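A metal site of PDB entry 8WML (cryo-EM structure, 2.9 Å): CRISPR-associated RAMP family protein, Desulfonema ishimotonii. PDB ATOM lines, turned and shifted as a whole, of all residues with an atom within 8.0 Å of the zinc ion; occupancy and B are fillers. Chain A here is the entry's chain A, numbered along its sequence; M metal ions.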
ATOM      1  N   ARG A 684     -24.747 -29.204 -23.273  1.00  0.00           N
ATOM      2  CA  ARG A 684     -23.993 -28.789 -22.091  1.00  0.00           C
ATOM      3  C   ARG A 684     -22.545 -29.271 -22.170  1.00  0.00           C
ATOM      4  O   ARG A 684     -21.618 -28.514 -21.867  1.00  0.00           O
ATOM      5  CB  ARG A 684     -24.673 -29.332 -20.837  1.00  0.00           C
ATOM      6  CG  ARG A 684     -23.980 -28.959 -19.538  1.00  0.00           C
ATOM      7  CD  ARG A 684     -24.851 -29.305 -18.348  1.00  0.00           C
ATOM      8  NE  ARG A 684     -24.285 -28.801 -17.102  1.00  0.00           N
ATOM      9  CZ  ARG A 684     -23.312 -29.406 -16.415  1.00  0.00           C
ATOM     10  NH1 ARG A 684     -22.774 -30.533 -16.821  1.00  0.00           N
ATOM     11  NH2 ARG A 684     -22.882 -28.839 -15.285  1.00  0.00           N
ATOM     12  N   CYS A 706     -20.630 -20.950  -6.553  1.00  0.00           N
ATOM     13  CA  CYS A 706     -20.061 -20.798  -7.877  1.00  0.00           C
ATOM     14  C   CYS A 706     -20.895 -19.830  -8.706  1.00  0.00           C
ATOM     15  O   CYS A 706     -22.098 -19.706  -8.494  1.00  0.00           O
ATOM     16  CB  CYS A 706     -19.958 -22.148  -8.582  1.00  0.00           C
ATOM     17  SG  CYS A 706     -19.351 -22.086 -10.280  1.00  0.00           S
ATOM     18  N   GLU A 707     -20.224 -19.115  -9.614  1.00  0.00           N
ATOM     19  CA  GLU A 707     -20.897 -18.110 -10.486  1.00  0.00           C
ATOM     20  C   GLU A 707     -20.332 -18.243 -11.898  1.00  0.00           C
ATOM     21  O   GLU A 707     -20.355 -17.236 -12.631  1.00  0.00           O
ATOM     22  CB  GLU A 707     -20.543 -16.700 -10.002  1.00  0.00           C
ATOM     23  CG  GLU A 707     -21.235 -15.585 -10.778  1.00  0.00           C
ATOM     24  CD  GLU A 707     -20.627 -15.193 -12.118  1.00  0.00           C
ATOM     25  OE1 GLU A 707     -19.411 -15.421 -12.310  1.00  0.00           O
ATOM     26  OE2 GLU A 707     -21.380 -14.654 -12.960  1.00  0.00           O
ATOM     27  N   CYS A 708     -19.823 -19.425 -12.252  1.00  0.00           N
ATOM     28  CA  CYS A 708     -19.238 -19.655 -13.561  1.00  0.00           C
ATOM     29  C   CYS A 708     -20.301 -19.606 -14.665  1.00  0.00           C
ATOM     30  O   CYS A 708     -21.514 -19.615 -14.398  1.00  0.00           O
ATOM     31  CB  CYS A 708     -18.525 -21.013 -13.592  1.00  0.00           C
ATOM     32  SG  CYS A 708     -19.610 -22.442 -13.407  1.00  0.00           S
ATOM     33  N   LEU A 709     -19.838 -19.545 -15.914  1.00  0.00           N
ATOM     34  CA  LEU A 709     -20.734 -19.391 -17.058  1.00  0.00           C
ATOM     35  C   LEU A 709     -21.696 -20.569 -17.163  1.00  0.00           C
ATOM     36  O   LEU A 709     -22.888 -20.379 -17.426  1.00  0.00           O
ATOM     37  CB  LEU A 709     -19.910 -19.244 -18.332  1.00  0.00           C
ATOM     38  CG  LEU A 709     -20.625 -18.850 -19.625  1.00  0.00           C
ATOM     39  CD1 LEU A 709     -19.790 -17.841 -20.398  1.00  0.00           C
ATOM     40  CD2 LEU A 709     -20.916 -20.063 -20.482  1.00  0.00           C
ATOM     41  N   LEU A 710     -21.184 -21.781 -16.961  1.00  0.00           N
ATOM     42  CA  LEU A 710     -22.031 -22.963 -17.057  1.00  0.00           C
ATOM     43  C   LEU A 710     -23.123 -22.935 -16.001  1.00  0.00           C
ATOM     44  O   LEU A 710     -24.291 -23.218 -16.291  1.00  0.00           O
ATOM     45  CB  LEU A 710     -21.168 -24.226 -16.901  1.00  0.00           C
ATOM     46  CG  LEU A 710     -21.685 -25.501 -17.586  1.00  0.00           C
ATOM     47  CD1 LEU A 710     -21.495 -25.421 -19.088  1.00  0.00           C
ATOM     48  CD2 LEU A 710     -20.970 -26.711 -17.024  1.00  0.00           C
ATOM     49  N   CYS A 711     -22.773 -22.568 -14.773  1.00  0.00           N
ATOM     50  CA  CYS A 711     -23.776 -22.482 -13.714  1.00  0.00           C
ATOM     51  C   CYS A 711     -24.814 -21.413 -14.042  1.00  0.00           C
ATOM     52  O   CYS A 711     -26.014 -21.646 -13.888  1.00  0.00           O
ATOM     53  CB  CYS A 711     -23.109 -22.182 -12.377  1.00  0.00           C
ATOM     54  SG  CYS A 711     -22.365 -23.632 -11.582  1.00  0.00           S
ATOM     55  N   GLN A 712     -24.367 -20.248 -14.511  1.00  0.00           N
ATOM     56  CA  GLN A 712     -25.308 -19.165 -14.783  1.00  0.00           C
ATOM     57  C   GLN A 712     -26.283 -19.541 -15.894  1.00  0.00           C
ATOM     58  O   GLN A 712     -27.468 -19.216 -15.817  1.00  0.00           O
ATOM     59  CB  GLN A 712     -24.561 -17.880 -15.154  1.00  0.00           C
ATOM     60  CG  GLN A 712     -23.820 -17.152 -14.030  1.00  0.00           C
ATOM     61  CD  GLN A 712     -24.616 -17.002 -12.746  1.00  0.00           C
ATOM     62  OE1 GLN A 712     -25.454 -16.105 -12.620  1.00  0.00           O
ATOM     63  NE2 GLN A 712     -24.376 -17.886 -11.789  1.00  0.00           N
ATOM     64  N   GLY A 715     -28.060 -23.452 -14.907  1.00  0.00           N
ATOM     65  CA  GLY A 715     -28.526 -23.677 -13.553  1.00  0.00           C
ATOM     66  C   GLY A 715     -27.636 -24.670 -12.813  1.00  0.00           C
ATOM     67  O   GLY A 715     -26.698 -25.238 -13.352  1.00  0.00           O
ATOM     68  N   SER A 716     -27.968 -24.869 -11.545  1.00  0.00           N
ATOM     69  CA  SER A 716     -27.233 -25.791 -10.679  1.00  0.00           C
ATOM     70  C   SER A 716     -28.162 -26.205  -9.540  1.00  0.00           C
ATOM     71  O   SER A 716     -29.367 -25.945  -9.575  1.00  0.00           O
ATOM     72  CB  SER A 716     -25.942 -25.138 -10.170  1.00  0.00           C
ATOM     73  OG  SER A 716     -26.212 -24.093  -9.263  1.00  0.00           O
ATOM     74  N   GLU A 719     -29.565 -22.917  -7.908  1.00  0.00           N
ATOM     75  CA  GLU A 719     -30.240 -21.904  -8.717  1.00  0.00           C
ATOM     76  C   GLU A 719     -30.846 -22.559  -9.943  1.00  0.00           C
ATOM     77  O   GLU A 719     -30.324 -23.546 -10.456  1.00  0.00           O
ATOM     78  CB  GLU A 719     -29.267 -20.786  -9.122  1.00  0.00           C
ATOM     79  CG  GLU A 719     -28.250 -21.180 -10.189  1.00  0.00           C
ATOM     80  CD  GLU A 719     -26.869 -20.621  -9.909  1.00  0.00           C
ATOM     81  OE1 GLU A 719     -26.693 -19.373  -9.965  1.00  0.00           O
ATOM     82  OE2 GLU A 719     -25.949 -21.412  -9.632  1.00  0.00           O
HETATM   83 ZN    ZN M   1     -20.069 -23.807 -11.618  1.00  0.00          ZN
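SG of Cys 706 is bound to the zinc ion (2.3 Å).
The side-chain sulfur (SG) of Cys 708 is bound to the zinc ion, 2.3 Å away.
The side-chain sulfur (SG) of Cys 711 is bound to the zinc ion, 2.3 Å away.
The zinc ion has three donor atoms within binding distance.
Of the 11 residues printed, 3 come within 4 Å of the zinc ion.
The nearest printed residue that does not touch the zinc ion is Glu 707 (5.1 Å).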
